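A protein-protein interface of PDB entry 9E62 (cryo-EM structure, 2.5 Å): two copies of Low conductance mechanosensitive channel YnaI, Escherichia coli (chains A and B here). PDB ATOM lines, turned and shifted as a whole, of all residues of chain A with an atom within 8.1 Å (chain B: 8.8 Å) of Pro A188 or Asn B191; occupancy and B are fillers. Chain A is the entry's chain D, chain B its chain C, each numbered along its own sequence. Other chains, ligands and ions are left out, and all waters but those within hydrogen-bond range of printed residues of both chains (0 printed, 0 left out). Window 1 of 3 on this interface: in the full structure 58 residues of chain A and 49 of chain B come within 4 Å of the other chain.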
ATOM      1  N   ARG A 186       0.931 -28.183 -16.030  1.00  0.00           N
ATOM      2  CA  ARG A 186       1.637 -29.029 -15.082  1.00  0.00           C
ATOM      3  C   ARG A 186       0.623 -29.652 -14.135  1.00  0.00           C
ATOM      4  O   ARG A 186      -0.535 -29.230 -14.078  1.00  0.00           O
ATOM      5  CB  ARG A 186       2.685 -28.229 -14.302  1.00  0.00           C
ATOM      6  CG  ARG A 186       3.931 -29.001 -13.946  1.00  0.00           C
ATOM      7  CD  ARG A 186       4.824 -28.185 -13.035  1.00  0.00           C
ATOM      8  NE  ARG A 186       4.212 -27.953 -11.734  1.00  0.00           N
ATOM      9  CZ  ARG A 186       4.176 -28.847 -10.754  1.00  0.00           C
ATOM     10  NH1 ARG A 186       4.709 -30.048 -10.894  1.00  0.00           N
ATOM     11  NH2 ARG A 186       3.588 -28.525  -9.605  1.00  0.00           N
ATOM     12  N   SER A 187       1.070 -30.665 -13.393  1.00  0.00           N
ATOM     13  CA  SER A 187       0.208 -31.313 -12.420  1.00  0.00           C
ATOM     14  C   SER A 187       1.043 -31.912 -11.298  1.00  0.00           C
ATOM     15  O   SER A 187       2.057 -32.568 -11.581  1.00  0.00           O
ATOM     16  CB  SER A 187      -0.647 -32.403 -13.064  1.00  0.00           C
ATOM     17  OG  SER A 187      -1.486 -33.019 -12.106  1.00  0.00           O
ATOM     18  N   PRO A 188       0.654 -31.711 -10.036  1.00  0.00           N
ATOM     19  CA  PRO A 188       1.388 -32.342  -8.928  1.00  0.00           C
ATOM     20  C   PRO A 188       1.075 -33.818  -8.743  1.00  0.00           C
ATOM     21  O   PRO A 188       1.734 -34.468  -7.922  1.00  0.00           O
ATOM     22  CB  PRO A 188       0.942 -31.529  -7.710  1.00  0.00           C
ATOM     23  CG  PRO A 188      -0.410 -31.031  -8.080  1.00  0.00           C
ATOM     24  CD  PRO A 188      -0.363 -30.763  -9.556  1.00  0.00           C
ATOM     25  N   ASP A 189       0.102 -34.367  -9.466  1.00  0.00           N
ATOM     26  CA  ASP A 189      -0.292 -35.764  -9.317  1.00  0.00           C
ATOM     27  C   ASP A 189       0.316 -36.678 -10.372  1.00  0.00           C
ATOM     28  O   ASP A 189       0.710 -37.802 -10.054  1.00  0.00           O
ATOM     29  CB  ASP A 189      -1.819 -35.888  -9.364  1.00  0.00           C
ATOM     30  CG  ASP A 189      -2.508 -34.971  -8.374  1.00  0.00           C
ATOM     31  OD1 ASP A 189      -2.049 -34.890  -7.217  1.00  0.00           O
ATOM     32  OD2 ASP A 189      -3.511 -34.333  -8.753  1.00  0.00           O
ATOM     33  N   ARG A 190       0.399 -36.225 -11.621  1.00  0.00           N
ATOM     34  CA  ARG A 190       0.932 -37.024 -12.712  1.00  0.00           C
ATOM     35  C   ARG A 190       1.934 -36.199 -13.503  1.00  0.00           C
ATOM     36  O   ARG A 190       1.995 -34.974 -13.380  1.00  0.00           O
ATOM     37  CB  ARG A 190      -0.178 -37.528 -13.645  1.00  0.00           C
ATOM     38  CG  ARG A 190      -1.345 -38.193 -12.937  1.00  0.00           C
ATOM     39  CD  ARG A 190      -1.132 -39.689 -12.805  1.00  0.00           C
ATOM     40  NE  ARG A 190      -1.063 -40.346 -14.103  1.00  0.00           N
ATOM     41  CZ  ARG A 190      -2.014 -41.122 -14.602  1.00  0.00           C
ATOM     42  NH1 ARG A 190      -3.132 -41.360 -13.937  1.00  0.00           N
ATOM     43  NH2 ARG A 190      -1.840 -41.672 -15.800  1.00  0.00           N
ATOM     44  N   ASN A 191       2.724 -36.888 -14.322  1.00  0.00           N
ATOM     45  CA  ASN A 191       3.731 -36.239 -15.161  1.00  0.00           C
ATOM     46  C   ASN A 191       3.100 -35.932 -16.514  1.00  0.00           C
ATOM     47  O   ASN A 191       3.023 -36.797 -17.388  1.00  0.00           O
ATOM     48  CB  ASN A 191       4.962 -37.124 -15.303  1.00  0.00           C
ATOM     49  CG  ASN A 191       6.155 -36.382 -15.864  1.00  0.00           C
ATOM     50  OD1 ASN A 191       6.041 -35.237 -16.296  1.00  0.00           O
ATOM     51  ND2 ASN A 191       7.311 -37.030 -15.855  1.00  0.00           N
ATOM     52  N   ILE A 192       2.639 -34.693 -16.684  1.00  0.00           N
ATOM     53  CA  ILE A 192       2.031 -34.249 -17.934  1.00  0.00           C
ATOM     54  C   ILE A 192       2.648 -32.922 -18.353  1.00  0.00           C
ATOM     55  O   ILE A 192       2.078 -32.197 -19.176  1.00  0.00           O
ATOM     56  CB  ILE A 192       0.502 -34.122 -17.800  1.00  0.00           C
ATOM     57  CG1 ILE A 192       0.142 -33.085 -16.734  1.00  0.00           C
ATOM     58  CG2 ILE A 192      -0.129 -35.464 -17.481  1.00  0.00           C
ATOM     59  CD1 ILE A 192      -1.244 -32.515 -16.883  1.00  0.00           C
ATOM     60  N   ILE A 224      -7.554 -35.036 -11.655  1.00  0.00           N
ATOM     61  CA  ILE A 224      -6.302 -34.520 -11.123  1.00  0.00           C
ATOM     62  C   ILE A 224      -6.336 -32.998 -11.158  1.00  0.00           C
ATOM     63  O   ILE A 224      -7.105 -32.384 -11.901  1.00  0.00           O
ATOM     64  CB  ILE A 224      -5.071 -35.046 -11.891  1.00  0.00           C
ATOM     65  CG1 ILE A 224      -4.959 -34.370 -13.257  1.00  0.00           C
ATOM     66  CG2 ILE A 224      -5.140 -36.555 -12.044  1.00  0.00           C
ATOM     67  CD1 ILE A 224      -3.707 -34.732 -14.015  1.00  0.00           C
ATOM     68  N   SER A 225      -5.490 -32.394 -10.331  1.00  0.00           N
ATOM     69  CA  SER A 225      -5.340 -30.946 -10.323  1.00  0.00           C
ATOM     70  C   SER A 225      -4.378 -30.516 -11.419  1.00  0.00           C
ATOM     71  O   SER A 225      -3.332 -31.134 -11.623  1.00  0.00           O
ATOM     72  CB  SER A 225      -4.835 -30.465  -8.963  1.00  0.00           C
ATOM     73  OG  SER A 225      -5.591 -31.027  -7.908  1.00  0.00           O
ATOM     74  N   VAL A 226      -4.737 -29.449 -12.124  1.00  0.00           N
ATOM     75  CA  VAL A 226      -3.953 -28.944 -13.244  1.00  0.00           C
ATOM     76  C   VAL A 226      -3.460 -27.550 -12.890  1.00  0.00           C
ATOM     77  O   VAL A 226      -4.259 -26.668 -12.554  1.00  0.00           O
ATOM     78  CB  VAL A 226      -4.764 -28.921 -14.547  1.00  0.00           C
ATOM     79  CG1 VAL A 226      -3.934 -28.336 -15.675  1.00  0.00           C
ATOM     80  CG2 VAL A 226      -5.231 -30.321 -14.901  1.00  0.00           C
ATOM     81  N   GLU A 227      -2.151 -27.355 -12.963  1.00  0.00           N
ATOM     82  CA  GLU A 227      -1.533 -26.054 -12.759  1.00  0.00           C
ATOM     83  C   GLU A 227      -1.160 -25.464 -14.111  1.00  0.00           C
ATOM     84  O   GLU A 227      -0.789 -26.195 -15.035  1.00  0.00           O
ATOM     85  CB  GLU A 227      -0.298 -26.175 -11.865  1.00  0.00           C
ATOM     86  CG  GLU A 227       0.398 -24.861 -11.565  1.00  0.00           C
ATOM     87  CD  GLU A 227       1.501 -25.014 -10.540  1.00  0.00           C
ATOM     88  OE1 GLU A 227       1.199 -25.418  -9.398  1.00  0.00           O
ATOM     89  OE2 GLU A 227       2.671 -24.738 -10.876  1.00  0.00           O
ATOM     90  N   ILE B 185      -5.890 -22.389   2.034  1.00  0.00           N
ATOM     91  CA  ILE B 185      -6.296 -23.735   2.408  1.00  0.00           C
ATOM     92  C   ILE B 185      -5.169 -24.707   2.093  1.00  0.00           C
ATOM     93  O   ILE B 185      -4.226 -24.398   1.363  1.00  0.00           O
ATOM     94  CB  ILE B 185      -7.600 -24.170   1.706  1.00  0.00           C
ATOM     95  CG1 ILE B 185      -7.404 -24.213   0.192  1.00  0.00           C
ATOM     96  CG2 ILE B 185      -8.737 -23.237   2.075  1.00  0.00           C
ATOM     97  CD1 ILE B 185      -8.489 -24.965  -0.534  1.00  0.00           C
ATOM     98  N   ARG B 186      -5.285 -25.909   2.656  1.00  0.00           N
ATOM     99  CA  ARG B 186      -4.232 -26.908   2.584  1.00  0.00           C
ATOM    100  C   ARG B 186      -4.847 -28.280   2.813  1.00  0.00           C
ATOM    101  O   ARG B 186      -5.991 -28.398   3.258  1.00  0.00           O
ATOM    102  CB  ARG B 186      -3.134 -26.628   3.612  1.00  0.00           C
ATOM    103  CG  ARG B 186      -1.742 -27.002   3.167  1.00  0.00           C
ATOM    104  CD  ARG B 186      -0.755 -26.850   4.306  1.00  0.00           C
ATOM    105  NE  ARG B 186      -1.010 -27.802   5.378  1.00  0.00           N
ATOM    106  CZ  ARG B 186      -0.648 -29.077   5.350  1.00  0.00           C
ATOM    107  NH1 ARG B 186      -0.010 -29.591   4.312  1.00  0.00           N
ATOM    108  NH2 ARG B 186      -0.933 -29.857   6.389  1.00  0.00           N
ATOM    109  N   SER B 187      -4.073 -29.321   2.499  1.00  0.00           N
ATOM    110  CA  SER B 187      -4.532 -30.682   2.715  1.00  0.00           C
ATOM    111  C   SER B 187      -3.344 -31.606   2.932  1.00  0.00           C
ATOM    112  O   SER B 187      -2.365 -31.525   2.174  1.00  0.00           O
ATOM    113  CB  SER B 187      -5.369 -31.185   1.542  1.00  0.00           C
ATOM    114  OG  SER B 187      -5.814 -32.510   1.770  1.00  0.00           O
ATOM    115  N   PRO B 188      -3.392 -32.482   3.939  1.00  0.00           N
ATOM    116  CA  PRO B 188      -2.299 -33.450   4.130  1.00  0.00           C
ATOM    117  C   PRO B 188      -2.337 -34.623   3.165  1.00  0.00           C
ATOM    118  O   PRO B 188      -1.391 -35.421   3.161  1.00  0.00           O
ATOM    119  CB  PRO B 188      -2.501 -33.919   5.573  1.00  0.00           C
ATOM    120  CG  PRO B 188      -3.958 -33.743   5.813  1.00  0.00           C
ATOM    121  CD  PRO B 188      -4.360 -32.518   5.048  1.00  0.00           C
ATOM    122  N   ASP B 189      -3.384 -34.758   2.355  1.00  0.00           N
ATOM    123  CA  ASP B 189      -3.521 -35.879   1.432  1.00  0.00           C
ATOM    124  C   ASP B 189      -3.106 -35.542   0.007  1.00  0.00           C
ATOM    125  O   ASP B 189      -2.484 -36.370  -0.663  1.00  0.00           O
ATOM    126  CB  ASP B 189      -4.967 -36.385   1.429  1.00  0.00           C
ATOM    127  CG  ASP B 189      -5.478 -36.700   2.819  1.00  0.00           C
ATOM    128  OD1 ASP B 189      -4.733 -37.326   3.601  1.00  0.00           O
ATOM    129  OD2 ASP B 189      -6.627 -36.325   3.131  1.00  0.00           O
ATOM    130  N   ARG B 190      -3.436 -34.346  -0.475  1.00  0.00           N
ATOM    131  CA  ARG B 190      -3.119 -33.930  -1.833  1.00  0.00           C
ATOM    132  C   ARG B 190      -2.502 -32.542  -1.805  1.00  0.00           C
ATOM    133  O   ARG B 190      -2.582 -31.822  -0.809  1.00  0.00           O
ATOM    134  CB  ARG B 190      -4.361 -33.931  -2.734  1.00  0.00           C
ATOM    135  CG  ARG B 190      -5.180 -35.208  -2.680  1.00  0.00           C
ATOM    136  CD  ARG B 190      -4.731 -36.198  -3.736  1.00  0.00           C
ATOM    137  NE  ARG B 190      -4.932 -35.685  -5.085  1.00  0.00           N
ATOM    138  CZ  ARG B 190      -5.865 -36.119  -5.920  1.00  0.00           C
ATOM    139  NH1 ARG B 190      -6.709 -37.077  -5.577  1.00  0.00           N
ATOM    140  NH2 ARG B 190      -5.953 -35.576  -7.131  1.00  0.00           N
ATOM    141  N   ASN B 191      -1.881 -32.170  -2.922  1.00  0.00           N
ATOM    142  CA  ASN B 191      -1.247 -30.859  -3.061  1.00  0.00           C
ATOM    143  C   ASN B 191      -2.264 -29.898  -3.665  1.00  0.00           C
ATOM    144  O   ASN B 191      -2.457 -29.861  -4.882  1.00  0.00           O
ATOM    145  CB  ASN B 191       0.009 -30.959  -3.917  1.00  0.00           C
ATOM    146  CG  ASN B 191       0.882 -29.728  -3.819  1.00  0.00           C
ATOM    147  OD1 ASN B 191       0.493 -28.721  -3.230  1.00  0.00           O
ATOM    148  ND2 ASN B 191       2.075 -29.803  -4.392  1.00  0.00           N
ATOM    149  N   ILE B 192      -2.925 -29.120  -2.806  1.00  0.00           N
ATOM    150  CA  ILE B 192      -3.911 -28.137  -3.241  1.00  0.00           C
ATOM    151  C   ILE B 192      -3.628 -26.803  -2.565  1.00  0.00           C
ATOM    152  O   ILE B 192      -4.499 -25.928  -2.512  1.00  0.00           O
ATOM    153  CB  ILE B 192      -5.345 -28.608  -2.938  1.00  0.00           C
ATOM    154  CG1 ILE B 192      -5.538 -28.802  -1.434  1.00  0.00           C
ATOM    155  CG2 ILE B 192      -5.667 -29.886  -3.691  1.00  0.00           C
ATOM    156  CD1 ILE B 192      -6.978 -28.746  -0.992  1.00  0.00           C
ATOM    157  N   GLU B 193      -2.414 -26.640  -2.042  1.00  0.00           N
ATOM    158  CA  GLU B 193      -2.100 -25.479  -1.221  1.00  0.00           C
ATOM    159  C   GLU B 193      -2.193 -24.186  -2.022  1.00  0.00           C
ATOM    160  O   GLU B 193      -1.732 -24.103  -3.162  1.00  0.00           O
ATOM    161  CB  GLU B 193      -0.700 -25.625  -0.623  1.00  0.00           C
ATOM    162  CG  GLU B 193      -0.302 -24.486   0.296  1.00  0.00           C
ATOM    163  CD  GLU B 193       0.505 -24.954   1.486  1.00  0.00           C
ATOM    164  OE1 GLU B 193       1.088 -26.054   1.414  1.00  0.00           O
ATOM    165  OE2 GLU B 193       0.557 -24.224   2.495  1.00  0.00           O
ATOM    166  N   GLY B 194      -2.787 -23.174  -1.409  1.00  0.00           N
ATOM    167  CA  GLY B 194      -2.945 -21.883  -2.043  1.00  0.00           C
ATOM    168  C   GLY B 194      -4.111 -21.137  -1.421  1.00  0.00           C
ATOM    169  O   GLY B 194      -4.677 -21.561  -0.416  1.00  0.00           O
ATOM    170  N   ILE B 206      -7.619 -21.945  -7.589  1.00  0.00           N
ATOM    171  CA  ILE B 206      -6.830 -21.570  -6.423  1.00  0.00           C
ATOM    172  C   ILE B 206      -5.532 -20.935  -6.904  1.00  0.00           C
ATOM    173  O   ILE B 206      -4.897 -21.443  -7.833  1.00  0.00           O
ATOM    174  CB  ILE B 206      -6.538 -22.794  -5.533  1.00  0.00           C
ATOM    175  CG1 ILE B 206      -7.776 -23.172  -4.720  1.00  0.00           C
ATOM    176  CG2 ILE B 206      -5.351 -22.545  -4.627  1.00  0.00           C
ATOM    177  CD1 ILE B 206      -7.812 -24.621  -4.312  1.00  0.00           C
ATOM    178  N   THR B 208      -1.765 -20.332  -6.337  1.00  0.00           N
ATOM    179  CA  THR B 208      -0.658 -20.885  -5.575  1.00  0.00           C
ATOM    180  C   THR B 208       0.245 -19.764  -5.067  1.00  0.00           C
ATOM    181  O   THR B 208       0.062 -18.585  -5.378  1.00  0.00           O
ATOM    182  CB  THR B 208       0.142 -21.870  -6.424  1.00  0.00           C
ATOM    183  OG1 THR B 208       0.721 -21.184  -7.540  1.00  0.00           O
ATOM    184  CG2 THR B 208      -0.753 -22.983  -6.932  1.00  0.00           C
ATOM    185  N   PHE B 209       1.241 -20.144  -4.271  1.00  0.00           N
ATOM    186  CA  PHE B 209       2.123 -19.166  -3.652  1.00  0.00           C
ATOM    187  C   PHE B 209       3.277 -18.745  -4.550  1.00  0.00           C
ATOM    188  O   PHE B 209       4.076 -17.898  -4.144  1.00  0.00           O
ATOM    189  CB  PHE B 209       2.657 -19.706  -2.324  1.00  0.00           C
ATOM    190  CG  PHE B 209       1.690 -19.557  -1.189  1.00  0.00           C
ATOM    191  CD1 PHE B 209       1.389 -18.306  -0.680  1.00  0.00           C
ATOM    192  CD2 PHE B 209       1.068 -20.664  -0.641  1.00  0.00           C
ATOM    193  CE1 PHE B 209       0.493 -18.165   0.360  1.00  0.00           C
ATOM    194  CE2 PHE B 209       0.172 -20.526   0.398  1.00  0.00           C
ATOM    195  CZ  PHE B 209      -0.115 -19.275   0.900  1.00  0.00           C
ATOM    196  N   PRO B 213      -2.163 -20.283 -11.384  1.00  0.00           N
ATOM    197  CA  PRO B 213      -3.502 -20.836 -11.155  1.00  0.00           C
ATOM    198  C   PRO B 213      -3.484 -22.355 -11.127  1.00  0.00           C
ATOM    199  O   PRO B 213      -2.775 -23.007 -11.895  1.00  0.00           O
ATOM    200  CB  PRO B 213      -4.305 -20.311 -12.349  1.00  0.00           C
ATOM    201  CG  PRO B 213      -3.296 -20.125 -13.418  1.00  0.00           C
ATOM    202  CD  PRO B 213      -2.013 -19.735 -12.745  1.00  0.00           C
ATOM    203  N   LEU B 214      -4.282 -22.919 -10.222  1.00  0.00           N
ATOM    204  CA  LEU B 214      -4.425 -24.359 -10.070  1.00  0.00           C
ATOM    205  C   LEU B 214      -5.908 -24.693 -10.058  1.00  0.00           C
ATOM    206  O   LEU B 214      -6.682 -24.064  -9.333  1.00  0.00           O
ATOM    207  CB  LEU B 214      -3.754 -24.846  -8.782  1.00  0.00           C
ATOM    208  CG  LEU B 214      -3.871 -26.328  -8.430  1.00  0.00           C
ATOM    209  CD1 LEU B 214      -2.958 -27.162  -9.306  1.00  0.00           C
ATOM    210  CD2 LEU B 214      -3.555 -26.550  -6.965  1.00  0.00           C
ATOM    211  N   TYR B 215      -6.301 -25.676 -10.859  1.00  0.00           N
ATOM    212  CA  TYR B 215      -7.695 -26.077 -10.985  1.00  0.00           C
ATOM    213  C   TYR B 215      -7.870 -27.436 -10.325  1.00  0.00           C
ATOM    214  O   TYR B 215      -7.232 -28.414 -10.729  1.00  0.00           O
ATOM    215  CB  TYR B 215      -8.114 -26.117 -12.453  1.00  0.00           C
ATOM    216  CG  TYR B 215      -7.834 -24.823 -13.180  1.00  0.00           C
ATOM    217  CD1 TYR B 215      -8.735 -23.771 -13.137  1.00  0.00           C
ATOM    218  CD2 TYR B 215      -6.658 -24.647 -13.895  1.00  0.00           C
ATOM    219  CE1 TYR B 215      -8.480 -22.585 -13.793  1.00  0.00           C
ATOM    220  CE2 TYR B 215      -6.393 -23.464 -14.554  1.00  0.00           C
ATOM    221  CZ  TYR B 215      -7.309 -22.438 -14.500  1.00  0.00           C
ATOM    222  OH  TYR B 215      -7.050 -21.258 -15.157  1.00  0.00           O
ATOM    223  N   VAL B 216      -8.732 -27.495  -9.317  1.00  0.00           N
ATOM    224  CA  VAL B 216      -8.929 -28.690  -8.507  1.00  0.00           C
ATOM    225  C   VAL B 216     -10.333 -29.220  -8.773  1.00  0.00           C
ATOM    226  O   VAL B 216     -11.308 -28.478  -8.627  1.00  0.00           O
ATOM    227  CB  VAL B 216      -8.736 -28.403  -7.009  1.00  0.00           C
ATOM    228  CG1 VAL B 216      -8.870 -29.682  -6.205  1.00  0.00           C
ATOM    229  CG2 VAL B 216      -7.387 -27.753  -6.766  1.00  0.00           C
ATOM    230  N   PRO B 217     -10.488 -30.478  -9.180  1.00  0.00           N
ATOM    231  CA  PRO B 217     -11.835 -31.040  -9.325  1.00  0.00           C
ATOM    232  C   PRO B 217     -12.575 -31.028  -7.998  1.00  0.00           C
ATOM    233  O   PRO B 217     -11.995 -31.273  -6.940  1.00  0.00           O
ATOM    234  CB  PRO B 217     -11.571 -32.469  -9.817  1.00  0.00           C
ATOM    235  CG  PRO B 217     -10.203 -32.420 -10.405  1.00  0.00           C
ATOM    236  CD  PRO B 217      -9.446 -31.440  -9.570  1.00  0.00           C
ATOM    237  N   LEU B 220     -12.734 -33.959  -5.127  1.00  0.00           N
ATOM    238  CA  LEU B 220     -11.683 -34.121  -4.129  1.00  0.00           C
ATOM    239  C   LEU B 220     -12.106 -33.585  -2.772  1.00  0.00           C
ATOM    240  O   LEU B 220     -11.675 -34.108  -1.739  1.00  0.00           O
ATOM    241  CB  LEU B 220     -10.404 -33.423  -4.587  1.00  0.00           C
ATOM    242  CG  LEU B 220      -9.722 -33.958  -5.844  1.00  0.00           C
ATOM    243  CD1 LEU B 220      -8.314 -33.405  -5.948  1.00  0.00           C
ATOM    244  CD2 LEU B 220      -9.702 -35.472  -5.836  1.00  0.00           C
ATOM    245  N   ILE B 224     -11.173 -35.948   1.022  1.00  0.00           N
ATOM    246  CA  ILE B 224      -9.908 -35.613   1.661  1.00  0.00           C
ATOM    247  C   ILE B 224     -10.165 -34.620   2.786  1.00  0.00           C
ATOM    248  O   ILE B 224     -11.188 -33.935   2.823  1.00  0.00           O
ATOM    249  CB  ILE B 224      -8.877 -35.041   0.665  1.00  0.00           C
ATOM    250  CG1 ILE B 224      -9.244 -33.610   0.274  1.00  0.00           C
ATOM    251  CG2 ILE B 224      -8.772 -35.924  -0.564  1.00  0.00           C
ATOM    252  CD1 ILE B 224      -8.212 -32.933  -0.593  1.00  0.00           C
ATOM    253  N   SER B 225      -9.218 -34.561   3.716  1.00  0.00           N
ATOM    254  CA  SER B 225      -9.277 -33.592   4.799  1.00  0.00           C
ATOM    255  C   SER B 225      -8.727 -32.253   4.331  1.00  0.00           C
ATOM    256  O   SER B 225      -7.701 -32.192   3.650  1.00  0.00           O
ATOM    257  CB  SER B 225      -8.488 -34.087   6.009  1.00  0.00           C
ATOM    258  OG  SER B 225      -8.836 -35.419   6.335  1.00  0.00           O
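Pro A188 touches Asn B191, but with the chains exchanged Asn A191 does not touch Pro B188 (18.0 Å). Asp A189 touches Arg B190, but with the chains exchanged Arg A190 does not touch Asp B189 (11.3 Å). Positions printed for both chains: 186, 187, 188, 189, 190, 191, 192, 224 and 225. Of the 11 pairs that touch across the chains among the printed residues, none has its exchanged pair printed and touching as well.
The backbone carbonyl oxygen of Ile B206 lies within hydrogen-bond range of the backbone NH of Leu B214, at 2.9 Å. The guanidinium group (NE) of Arg A186 lies within salt-bridge range of the side-chain carboxylate (OE2) of Glu A227 (3.7 Å). OG of Ser A187 lies close to N of Asp A189 (3.4 Å). O of Ser A225 lies within hydrogen-bond range of OG of Ser A187 (2.7 Å). OD2 of Asp A189 is in hydrogen-bond range of N of Ser A225, 3.2 Å away.
Pro A188 touches just one residue of chain B: Asn B191 (3.9 Å). Asn B191 touches just one residue of chain A: Pro A188 (3.9 Å). Of the printed residues of chain A, Tyr B215 touches Ser A225 and Val A226. Of the printed residues of chain A, Thr B208 touches Glu A227. Of the printed residues of chain B, Glu A227 touches Thr B208 (3.98 Å), Pro B213 (3.4 Å) and Leu B214 (3.7 Å). Of the printed residues of chain A, Val B216 touches Ser A225. Ser B187 touches none of the printed residues of chain A. The nearest residue of chain A that does not touch Asn B191 is Ser A225 (4.5 Å). The nearest printed residue of chain A that does not touch Leu B214 is Pro A188 (4.4 Å).
Among the printed residues, merely in contact across the chains: Pro A188 with Asn B191 (3.9 Å), Ile A224 with Pro B217 (3.4 Å), Ser A225 with Leu B214 (3.8 Å), Ser A225 with Tyr B215 (3.2 Å), Ser A225 with Val B216 (3.9 Å), Val A226 with Leu B214 (3.4 Å), Glu A227 with Thr B208 (3.98 Å), Glu A227 with Pro B213 (3.4 Å) and Glu A227 with Leu B214 (3.7 Å).
NH2 of Arg B190 lies within salt-bridge range of OD2 of Asp A189, 3.2 Å away. N of Tyr B215 sits at hydrogen-bond distance from O of Val A226, at 2.8 Å.
Of the 11 printed residues of chain A, 6 touch a printed residue of chain B. Hydrophobic or aromatic side chains of chain A within 4 Å of the printed part of chain B: Pro A188.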
